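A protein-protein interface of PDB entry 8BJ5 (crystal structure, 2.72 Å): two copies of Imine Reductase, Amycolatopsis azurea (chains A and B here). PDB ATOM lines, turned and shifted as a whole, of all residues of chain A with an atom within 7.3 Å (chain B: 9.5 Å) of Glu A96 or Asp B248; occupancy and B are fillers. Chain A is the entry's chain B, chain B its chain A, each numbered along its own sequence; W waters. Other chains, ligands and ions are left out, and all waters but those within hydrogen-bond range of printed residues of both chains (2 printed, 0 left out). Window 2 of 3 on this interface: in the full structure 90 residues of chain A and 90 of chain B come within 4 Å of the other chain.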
ATOM      1  N   TYR A  72      18.446 -39.712   8.676  1.00  0.00           N
ATOM      2  CA  TYR A  72      18.585 -40.706   9.767  1.00  0.00           C
ATOM      3  C   TYR A  72      17.372 -41.647   9.717  1.00  0.00           C
ATOM      4  O   TYR A  72      17.576 -42.878   9.740  1.00  0.00           O
ATOM      5  CB  TYR A  72      18.808 -39.977  11.096  1.00  0.00           C
ATOM      6  CG  TYR A  72      20.167 -39.332  11.277  1.00  0.00           C
ATOM      7  CD1 TYR A  72      21.334 -40.070  11.208  1.00  0.00           C
ATOM      8  CD2 TYR A  72      20.286 -37.984  11.566  1.00  0.00           C
ATOM      9  CE1 TYR A  72      22.576 -39.482  11.395  1.00  0.00           C
ATOM     10  CE2 TYR A  72      21.518 -37.375  11.763  1.00  0.00           C
ATOM     11  CZ  TYR A  72      22.672 -38.134  11.692  1.00  0.00           C
ATOM     12  OH  TYR A  72      23.902 -37.569  11.888  1.00  0.00           O
ATOM     13  N   ASP A  93      20.736 -28.262   6.609  1.00  0.00           N
ATOM     14  CA  ASP A  93      20.770 -28.444   8.084  1.00  0.00           C
ATOM     15  C   ASP A  93      21.998 -27.683   8.607  1.00  0.00           C
ATOM     16  O   ASP A  93      22.583 -26.926   7.824  1.00  0.00           O
ATOM     17  CB  ASP A  93      20.735 -29.937   8.460  1.00  0.00           C
ATOM     18  CG  ASP A  93      20.056 -30.191   9.780  1.00  0.00           C
ATOM     19  OD1 ASP A  93      20.505 -29.602  10.759  1.00  0.00           O
ATOM     20  OD2 ASP A  93      19.077 -30.932   9.803  1.00  0.00           O
ATOM     21  N   THR A  94      22.363 -27.857   9.880  1.00  0.00           N
ATOM     22  CA  THR A  94      23.457 -27.082  10.517  1.00  0.00           C
ATOM     23  C   THR A  94      24.800 -27.677  10.091  1.00  0.00           C
ATOM     24  O   THR A  94      24.923 -28.883   9.879  1.00  0.00           O
ATOM     25  CB  THR A  94      23.289 -27.000  12.041  1.00  0.00           C
ATOM     26  OG1 THR A  94      23.509 -28.282  12.636  1.00  0.00           O
ATOM     27  CG2 THR A  94      21.939 -26.435  12.432  1.00  0.00           C
ATOM     28  N   PRO A  95      25.850 -26.838   9.926  1.00  0.00           N
ATOM     29  CA  PRO A  95      27.207 -27.342   9.756  1.00  0.00           C
ATOM     30  C   PRO A  95      27.571 -28.402  10.811  1.00  0.00           C
ATOM     31  O   PRO A  95      28.060 -29.466  10.432  1.00  0.00           O
ATOM     32  CB  PRO A  95      28.068 -26.079   9.910  1.00  0.00           C
ATOM     33  CG  PRO A  95      27.184 -24.984   9.390  1.00  0.00           C
ATOM     34  CD  PRO A  95      25.801 -25.369   9.878  1.00  0.00           C
ATOM     35  N   GLU A  96      27.316 -28.119  12.093  1.00  0.00           N
ATOM     36  CA  GLU A  96      27.630 -29.070  13.203  1.00  0.00           C
ATOM     37  C   GLU A  96      26.914 -30.409  12.957  1.00  0.00           C
ATOM     38  O   GLU A  96      27.595 -31.450  13.061  1.00  0.00           O
ATOM     39  CB  GLU A  96      27.321 -28.453  14.573  1.00  0.00           C
ATOM     40  CG  GLU A  96      28.561 -27.955  15.314  1.00  0.00           C
ATOM     41  CD  GLU A  96      29.728 -27.473  14.451  1.00  0.00           C
ATOM     42  OE1 GLU A  96      30.742 -28.209  14.388  1.00  0.00           O
ATOM     43  OE2 GLU A  96      29.624 -26.369  13.825  1.00  0.00           O
ATOM     44  N   LYS A  97      25.624 -30.385  12.584  1.00  0.00           N
ATOM     45  CA  LYS A  97      24.853 -31.627  12.318  1.00  0.00           C
ATOM     46  C   LYS A  97      25.350 -32.288  11.028  1.00  0.00           C
ATOM     47  O   LYS A  97      25.206 -33.518  10.934  1.00  0.00           O
ATOM     48  CB  LYS A  97      23.346 -31.356  12.322  1.00  0.00           C
ATOM     49  CG  LYS A  97      22.655 -31.718  13.631  1.00  0.00           C
ATOM     50  CD  LYS A  97      21.414 -30.928  13.944  1.00  0.00           C
ATOM     51  CE  LYS A  97      20.577 -31.538  15.042  1.00  0.00           C
ATOM     52  NZ  LYS A  97      19.174 -31.060  14.956  1.00  0.00           N
ATOM     53  N   THR A  98      25.939 -31.515  10.112  1.00  0.00           N
ATOM     54  CA  THR A  98      26.528 -32.022   8.843  1.00  0.00           C
ATOM     55  C   THR A  98      27.756 -32.892   9.128  1.00  0.00           C
ATOM     56  O   THR A  98      27.886 -33.956   8.495  1.00  0.00           O
ATOM     57  CB  THR A  98      26.900 -30.882   7.891  1.00  0.00           C
ATOM     58  OG1 THR A  98      25.729 -30.102   7.688  1.00  0.00           O
ATOM     59  CG2 THR A  98      27.374 -31.377   6.550  1.00  0.00           C
ATOM     60  N   ARG A  99      28.640 -32.446  10.024  1.00  0.00           N
ATOM     61  CA  ARG A  99      29.864 -33.213  10.379  1.00  0.00           C
ATOM     62  C   ARG A  99      29.413 -34.488  11.091  1.00  0.00           C
ATOM     63  O   ARG A  99      29.811 -35.591  10.654  1.00  0.00           O
ATOM     64  CB  ARG A  99      30.824 -32.404  11.257  1.00  0.00           C
ATOM     65  CG  ARG A  99      31.989 -33.216  11.809  1.00  0.00           C
ATOM     66  N   GLU A 100      28.578 -34.331  12.124  1.00  0.00           N
ATOM     67  CA  GLU A 100      28.013 -35.452  12.918  1.00  0.00           C
ATOM     68  C   GLU A 100      27.440 -36.508  11.958  1.00  0.00           C
ATOM     69  O   GLU A 100      27.557 -37.702  12.275  1.00  0.00           O
ATOM     70  CB  GLU A 100      27.000 -34.902  13.925  1.00  0.00           C
ATOM     71  CG  GLU A 100      25.810 -35.807  14.164  1.00  0.00           C
ATOM     72  CD  GLU A 100      24.718 -35.194  15.012  1.00  0.00           C
ATOM     73  OE1 GLU A 100      23.611 -35.757  15.012  1.00  0.00           O
ATOM     74  OE2 GLU A 100      24.978 -34.164  15.666  1.00  0.00           O
ATOM     75  N   ALA A 101      26.865 -36.082  10.828  1.00  0.00           N
ATOM     76  CA  ALA A 101      26.307 -36.963   9.777  1.00  0.00           C
ATOM     77  C   ALA A 101      27.452 -37.624   9.004  1.00  0.00           C
ATOM     78  O   ALA A 101      27.403 -38.843   8.814  1.00  0.00           O
ATOM     79  CB  ALA A 101      25.393 -36.185   8.867  1.00  0.00           C
ATOM     80  N   ALA A 102      28.441 -36.851   8.565  1.00  0.00           N
ATOM     81  CA  ALA A 102      29.644 -37.384   7.895  1.00  0.00           C
ATOM     82  C   ALA A 102      30.169 -38.591   8.684  1.00  0.00           C
ATOM     83  O   ALA A 102      30.382 -39.661   8.067  1.00  0.00           O
ATOM     84  CB  ALA A 102      30.678 -36.310   7.748  1.00  0.00           C
ATOM     85  N   GLU A 103      30.300 -38.449  10.009  1.00  0.00           N
ATOM     86  CA  GLU A 103      30.916 -39.471  10.907  1.00  0.00           C
ATOM     87  C   GLU A 103      30.005 -40.702  11.007  1.00  0.00           C
ATOM     88  O   GLU A 103      30.506 -41.826  10.919  1.00  0.00           O
ATOM     89  CB  GLU A 103      31.182 -38.867  12.286  1.00  0.00           C
ATOM     90  CG  GLU A 103      32.308 -37.838  12.295  1.00  0.00           C
ATOM     91  CD  GLU A 103      32.510 -37.108  13.626  1.00  0.00           C
ATOM     92  OE1 GLU A 103      32.160 -37.677  14.715  1.00  0.00           O
ATOM     93  OE2 GLU A 103      33.019 -35.952  13.586  1.00  0.00           O
ATOM     94  N   ARG A 161      31.715 -29.727   6.430  1.00  0.00           N
ATOM     95  CA  ARG A 161      30.824 -28.614   6.855  1.00  0.00           C
ATOM     96  C   ARG A 161      30.807 -27.451   5.856  1.00  0.00           C
ATOM     97  O   ARG A 161      29.837 -26.728   5.873  1.00  0.00           O
ATOM     98  CB  ARG A 161      31.259 -28.083   8.221  1.00  0.00           C
ATOM     99  CG  ARG A 161      31.288 -29.136   9.322  1.00  0.00           C
ATOM    100  CD  ARG A 161      31.854 -28.556  10.602  1.00  0.00           C
ATOM    101  NE  ARG A 161      32.912 -27.610  10.257  1.00  0.00           N
ATOM    102  CZ  ARG A 161      33.759 -27.064  11.109  1.00  0.00           C
ATOM    103  NH1 ARG A 161      33.666 -27.338  12.400  1.00  0.00           N
ATOM    104  NH2 ARG A 161      34.686 -26.236  10.651  1.00  0.00           N
ATOM    105  N   GLN A 164      27.638 -26.779   3.563  1.00  0.00           N
ATOM    106  CA  GLN A 164      26.476 -26.460   4.430  1.00  0.00           C
ATOM    107  C   GLN A 164      26.614 -25.028   4.938  1.00  0.00           C
ATOM    108  O   GLN A 164      25.636 -24.289   4.867  1.00  0.00           O
ATOM    109  CB  GLN A 164      26.386 -27.421   5.615  1.00  0.00           C
ATOM    110  CG  GLN A 164      25.066 -27.344   6.348  1.00  0.00           C
ATOM    111  CD  GLN A 164      23.938 -27.892   5.504  1.00  0.00           C
ATOM    112  OE1 GLN A 164      23.664 -29.098   5.505  1.00  0.00           O
ATOM    113  NE2 GLN A 164      23.277 -27.001   4.772  1.00  0.00           N
ATOM    114  N   LEU A 165      27.801 -24.666   5.417  1.00  0.00           N
ATOM    115  CA  LEU A 165      28.114 -23.304   5.911  1.00  0.00           C
ATOM    116  C   LEU A 165      27.840 -22.270   4.806  1.00  0.00           C
ATOM    117  O   LEU A 165      27.250 -21.225   5.104  1.00  0.00           O
ATOM    118  CB  LEU A 165      29.575 -23.255   6.366  1.00  0.00           C
ATOM    119  CG  LEU A 165      30.021 -21.918   6.943  1.00  0.00           C
ATOM    120  CD1 LEU A 165      29.467 -21.763   8.343  1.00  0.00           C
ATOM    121  CD2 LEU A 165      31.527 -21.800   6.958  1.00  0.00           C
ATOM    122  N   ALA B 186      29.392 -12.872   8.770  1.00  0.00           N
ATOM    123  CA  ALA B 186      29.744 -13.177  10.180  1.00  0.00           C
ATOM    124  C   ALA B 186      29.685 -14.687  10.426  1.00  0.00           C
ATOM    125  O   ALA B 186      30.480 -15.189  11.229  1.00  0.00           O
ATOM    126  CB  ALA B 186      28.820 -12.451  11.129  1.00  0.00           C
ATOM    127  N   LEU B 187      28.774 -15.397   9.757  1.00  0.00           N
ATOM    128  CA  LEU B 187      28.673 -16.880   9.870  1.00  0.00           C
ATOM    129  C   LEU B 187      29.917 -17.496   9.242  1.00  0.00           C
ATOM    130  O   LEU B 187      30.542 -18.347   9.915  1.00  0.00           O
ATOM    131  CB  LEU B 187      27.400 -17.402   9.209  1.00  0.00           C
ATOM    132  CG  LEU B 187      27.097 -18.883   9.437  1.00  0.00           C
ATOM    133  CD1 LEU B 187      26.837 -19.245  10.907  1.00  0.00           C
ATOM    134  CD2 LEU B 187      25.868 -19.284   8.627  1.00  0.00           C
ATOM    135  N   SER B 190      33.151 -16.878  11.189  1.00  0.00           N
ATOM    136  CA  SER B 190      33.147 -17.662  12.451  1.00  0.00           C
ATOM    137  C   SER B 190      33.978 -18.934  12.278  1.00  0.00           C
ATOM    138  O   SER B 190      34.655 -19.307  13.251  1.00  0.00           O
ATOM    139  CB  SER B 190      31.749 -17.994  12.897  1.00  0.00           C
ATOM    140  OG  SER B 190      31.310 -19.203  12.312  1.00  0.00           O
ATOM    141  N   ALA B 191      33.912 -19.572  11.098  1.00  0.00           N
ATOM    142  CA  ALA B 191      34.683 -20.787  10.727  1.00  0.00           C
ATOM    143  C   ALA B 191      36.021 -20.405  10.079  1.00  0.00           C
ATOM    144  O   ALA B 191      36.751 -21.331   9.653  1.00  0.00           O
ATOM    145  CB  ALA B 191      33.856 -21.654   9.809  1.00  0.00           C
ATOM    146  N   ASP B 240      15.107 -22.312  10.487  1.00  0.00           N
ATOM    147  CA  ASP B 240      15.492 -22.985  11.767  1.00  0.00           C
ATOM    148  C   ASP B 240      16.994 -23.292  11.762  1.00  0.00           C
ATOM    149  O   ASP B 240      17.652 -23.029  12.788  1.00  0.00           O
ATOM    150  CB  ASP B 240      14.693 -24.270  12.007  1.00  0.00           C
ATOM    151  CG  ASP B 240      13.213 -24.032  12.257  1.00  0.00           C
ATOM    152  OD1 ASP B 240      12.838 -22.864  12.530  1.00  0.00           O
ATOM    153  OD2 ASP B 240      12.444 -25.003  12.160  1.00  0.00           O
ATOM    154  N   HIS B 241      17.507 -23.792  10.632  1.00  0.00           N
ATOM    155  CA  HIS B 241      18.936 -24.132  10.399  1.00  0.00           C
ATOM    156  C   HIS B 241      19.813 -22.889  10.526  1.00  0.00           C
ATOM    157  O   HIS B 241      20.831 -22.970  11.221  1.00  0.00           O
ATOM    158  CB  HIS B 241      19.087 -24.813   9.033  1.00  0.00           C
ATOM    159  CG  HIS B 241      18.227 -26.026   8.895  1.00  0.00           C
ATOM    160  ND1 HIS B 241      17.821 -26.507   7.677  1.00  0.00           N
ATOM    161  CD2 HIS B 241      17.691 -26.841   9.835  1.00  0.00           C
ATOM    162  CE1 HIS B 241      17.076 -27.573   7.869  1.00  0.00           C
ATOM    163  NE2 HIS B 241      16.988 -27.802   9.181  1.00  0.00           N
ATOM    164  N   ILE B 242      19.436 -21.781   9.886  1.00  0.00           N
ATOM    165  CA  ILE B 242      20.233 -20.521   9.930  1.00  0.00           C
ATOM    166  C   ILE B 242      20.273 -20.032  11.377  1.00  0.00           C
ATOM    167  O   ILE B 242      21.339 -19.612  11.827  1.00  0.00           O
ATOM    168  CB  ILE B 242      19.670 -19.460   8.961  1.00  0.00           C
ATOM    169  CG1 ILE B 242      19.752 -19.950   7.507  1.00  0.00           C
ATOM    170  CG2 ILE B 242      20.371 -18.115   9.150  1.00  0.00           C
ATOM    171  CD1 ILE B 242      18.695 -19.368   6.596  1.00  0.00           C
ATOM    172  N   VAL B 243      19.149 -20.095  12.082  1.00  0.00           N
ATOM    173  CA  VAL B 243      19.079 -19.706  13.517  1.00  0.00           C
ATOM    174  C   VAL B 243      20.053 -20.583  14.307  1.00  0.00           C
ATOM    175  O   VAL B 243      20.937 -20.016  14.999  1.00  0.00           O
ATOM    176  CB  VAL B 243      17.651 -19.786  14.076  1.00  0.00           C
ATOM    177  CG1 VAL B 243      17.638 -19.885  15.595  1.00  0.00           C
ATOM    178  CG2 VAL B 243      16.837 -18.589  13.614  1.00  0.00           C
ATOM    179  N   GLN B 244      19.943 -21.905  14.172  1.00  0.00           N
ATOM    180  CA  GLN B 244      20.717 -22.851  15.019  1.00  0.00           C
ATOM    181  C   GLN B 244      22.213 -22.756  14.681  1.00  0.00           C
ATOM    182  O   GLN B 244      23.015 -22.775  15.624  1.00  0.00           O
ATOM    183  CB  GLN B 244      20.156 -24.266  14.882  1.00  0.00           C
ATOM    184  CG  GLN B 244      20.779 -25.258  15.862  1.00  0.00           C
ATOM    185  CD  GLN B 244      20.665 -24.844  17.316  1.00  0.00           C
ATOM    186  OE1 GLN B 244      19.567 -24.646  17.842  1.00  0.00           O
ATOM    187  NE2 GLN B 244      21.807 -24.717  17.980  1.00  0.00           N
ATOM    188  N   ALA B 245      22.572 -22.649  13.391  1.00  0.00           N
ATOM    189  CA  ALA B 245      23.954 -22.387  12.898  1.00  0.00           C
ATOM    190  C   ALA B 245      24.499 -21.089  13.512  1.00  0.00           C
ATOM    191  O   ALA B 245      25.697 -21.061  13.903  1.00  0.00           O
ATOM    192  CB  ALA B 245      23.978 -22.311  11.390  1.00  0.00           C
ATOM    193  N   SER B 246      23.654 -20.050  13.593  1.00  0.00           N
ATOM    194  CA  SER B 246      24.000 -18.740  14.199  1.00  0.00           C
ATOM    195  C   SER B 246      24.325 -18.924  15.694  1.00  0.00           C
ATOM    196  O   SER B 246      25.388 -18.447  16.129  1.00  0.00           O
ATOM    197  CB  SER B 246      22.902 -17.739  13.944  1.00  0.00           C
ATOM    198  OG  SER B 246      22.793 -17.513  12.553  1.00  0.00           O
ATOM    199  N   ARG B 247      23.469 -19.614  16.450  1.00  0.00           N
ATOM    200  CA  ARG B 247      23.740 -19.956  17.880  1.00  0.00           C
ATOM    201  C   ARG B 247      25.025 -20.791  17.975  1.00  0.00           C
ATOM    202  O   ARG B 247      25.884 -20.437  18.794  1.00  0.00           O
ATOM    203  CB  ARG B 247      22.568 -20.709  18.525  1.00  0.00           C
ATOM    204  CG  ARG B 247      21.195 -20.094  18.288  1.00  0.00           C
ATOM    205  CD  ARG B 247      20.457 -19.515  19.495  1.00  0.00           C
ATOM    206  NE  ARG B 247      19.028 -19.541  19.207  1.00  0.00           N
ATOM    207  CZ  ARG B 247      18.171 -20.450  19.650  1.00  0.00           C
ATOM    208  NH1 ARG B 247      18.591 -21.431  20.438  1.00  0.00           N
ATOM    209  NH2 ARG B 247      16.896 -20.387  19.293  1.00  0.00           N
ATOM    210  N   ASP B 248      25.163 -21.844  17.168  1.00  0.00           N
ATOM    211  CA  ASP B 248      26.382 -22.704  17.126  1.00  0.00           C
ATOM    212  C   ASP B 248      27.631 -21.818  16.934  1.00  0.00           C
ATOM    213  O   ASP B 248      28.601 -22.024  17.665  1.00  0.00           O
ATOM    214  CB  ASP B 248      26.253 -23.796  16.057  1.00  0.00           C
ATOM    215  CG  ASP B 248      25.335 -24.947  16.457  1.00  0.00           C
ATOM    216  OD1 ASP B 248      24.836 -24.956  17.634  1.00  0.00           O
ATOM    217  OD2 ASP B 248      25.114 -25.831  15.607  1.00  0.00           O
ATOM    218  N   ALA B 249      27.596 -20.846  16.014  1.00  0.00           N
ATOM    219  CA  ALA B 249      28.740 -19.967  15.669  1.00  0.00           C
ATOM    220  C   ALA B 249      28.913 -18.835  16.694  1.00  0.00           C
ATOM    221  O   ALA B 249      30.002 -18.229  16.704  1.00  0.00           O
ATOM    222  CB  ALA B 249      28.573 -19.407  14.275  1.00  0.00           C
ATOM    223  N   GLY B 250      27.894 -18.531  17.504  1.00  0.00           N
ATOM    224  CA  GLY B 250      27.932 -17.457  18.523  1.00  0.00           C
ATOM    225  C   GLY B 250      27.806 -16.056  17.932  1.00  0.00           C
ATOM    226  O   GLY B 250      28.256 -15.104  18.564  1.00  0.00           O
ATOM    227  N   ILE B 251      27.218 -15.914  16.747  1.00  0.00           N
ATOM    228  CA  ILE B 251      26.928 -14.592  16.104  1.00  0.00           C
ATOM    229  C   ILE B 251      25.522 -14.120  16.510  1.00  0.00           C
ATOM    230  O   ILE B 251      24.883 -14.821  17.313  1.00  0.00           O
ATOM    231  CB  ILE B 251      27.069 -14.702  14.577  1.00  0.00           C
ATOM    232  CG1 ILE B 251      25.999 -15.630  13.991  1.00  0.00           C
ATOM    233  CG2 ILE B 251      28.479 -15.120  14.230  1.00  0.00           C
ATOM    234  CD1 ILE B 251      25.987 -15.698  12.490  1.00  0.00           C
ATOM    235  N   ASP B 252      25.067 -12.989  15.959  1.00  0.00           N
ATOM    236  CA  ASP B 252      23.719 -12.407  16.199  1.00  0.00           C
ATOM    237  C   ASP B 252      22.631 -13.422  15.833  1.00  0.00           C
ATOM    238  O   ASP B 252      22.781 -14.070  14.788  1.00  0.00           O
ATOM    239  CB  ASP B 252      23.493 -11.122  15.401  1.00  0.00           C
ATOM    240  CG  ASP B 252      22.065 -10.617  15.491  1.00  0.00           C
ATOM    241  OD1 ASP B 252      21.655 -10.200  16.568  1.00  0.00           O
ATOM    242  OD2 ASP B 252      21.372 -10.667  14.488  1.00  0.00           O
ATOM    243  N   VAL B 253      21.565 -13.507  16.629  1.00  0.00           N
ATOM    244  CA  VAL B 253      20.418 -14.417  16.357  1.00  0.00           C
ATOM    245  C   VAL B 253      19.131 -13.615  16.118  1.00  0.00           C
ATOM    246  O   VAL B 253      18.152 -14.214  15.644  1.00  0.00           O
ATOM    247  CB  VAL B 253      20.252 -15.449  17.496  1.00  0.00           C
ATOM    248  CG1 VAL B 253      21.379 -16.470  17.470  1.00  0.00           C
ATOM    249  CG2 VAL B 253      20.133 -14.806  18.876  1.00  0.00           C
HETATM  250  O   HOH W   1      23.838 -28.014  15.149  1.00  0.00           O
HETATM  251  O   HOH W   2      26.858 -25.110  13.299  1.00  0.00           O
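The backbone carbonyl oxygen (O) of Asp A93 lies close to the side-chain amide nitrogen (NE2) of Gln A164. NH1 of Arg A161 lies within salt-bridge range of OE1 of Glu A96 (3.6 Å). O of Leu B187 is in hydrogen-bond range of OG of Ser B190 (2.7 Å). The backbone carbonyl oxygen (O) of Thr A94 is in hydrogen-bond range of the side-chain hydroxyl (OG1) of Thr A98. OG1 of Thr A94 sits at hydrogen-bond distance from N of Lys A97. OD1 of Asp B248 sits at hydrogen-bond distance from NE2 of Gln B244, 3.1 Å away.
Among the printed residues, merely in contact across the chains: Asp A93 with His B241, Glu A96 with Asp B248, Leu A165 with Ala B191, Thr A94 with Gln B244, Thr A94 with His B241, Pro A95 with Ala B245, Leu A165 with Leu B187 and Thr A94 with Ala B245.
Printed residues of chain B within 4 Å of Glu A96: Asp B248. Thr A94 touches three residues of chain B. Pro A95 touches one residue of chain B. No residue of chain B comes within 4 Å of Arg A99. Printed residues of chain A within 4 Å of Leu B187: Leu A165. Printed residues of chain A within 4 Å of Gln B244: Thr A94 (3.7 Å). Printed residues of chain A within 4 Å of His B241: Asp A93 and Thr A94. Printed residues of chain A within 4 Å of Ala B245: Thr A94 and Pro A95.
Of the 15 printed residues of chain A, 5 touch a printed residue of chain B. Hydrophobic or aromatic side chains of chain A that line the printed part of chain B: Pro A95 and Leu A165.
No position is printed for both chains. Of the 8 pairs that touch across the chains among the printed residues, none has its exchanged pair printed and touching as well.
Water W1 bridges OG1 of Thr A94 and OD2 of Asp B248. Water W2 bridges OD2 of Asp B248 (3.0 Å) and OE2 of Glu A96 (3.1 Å).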
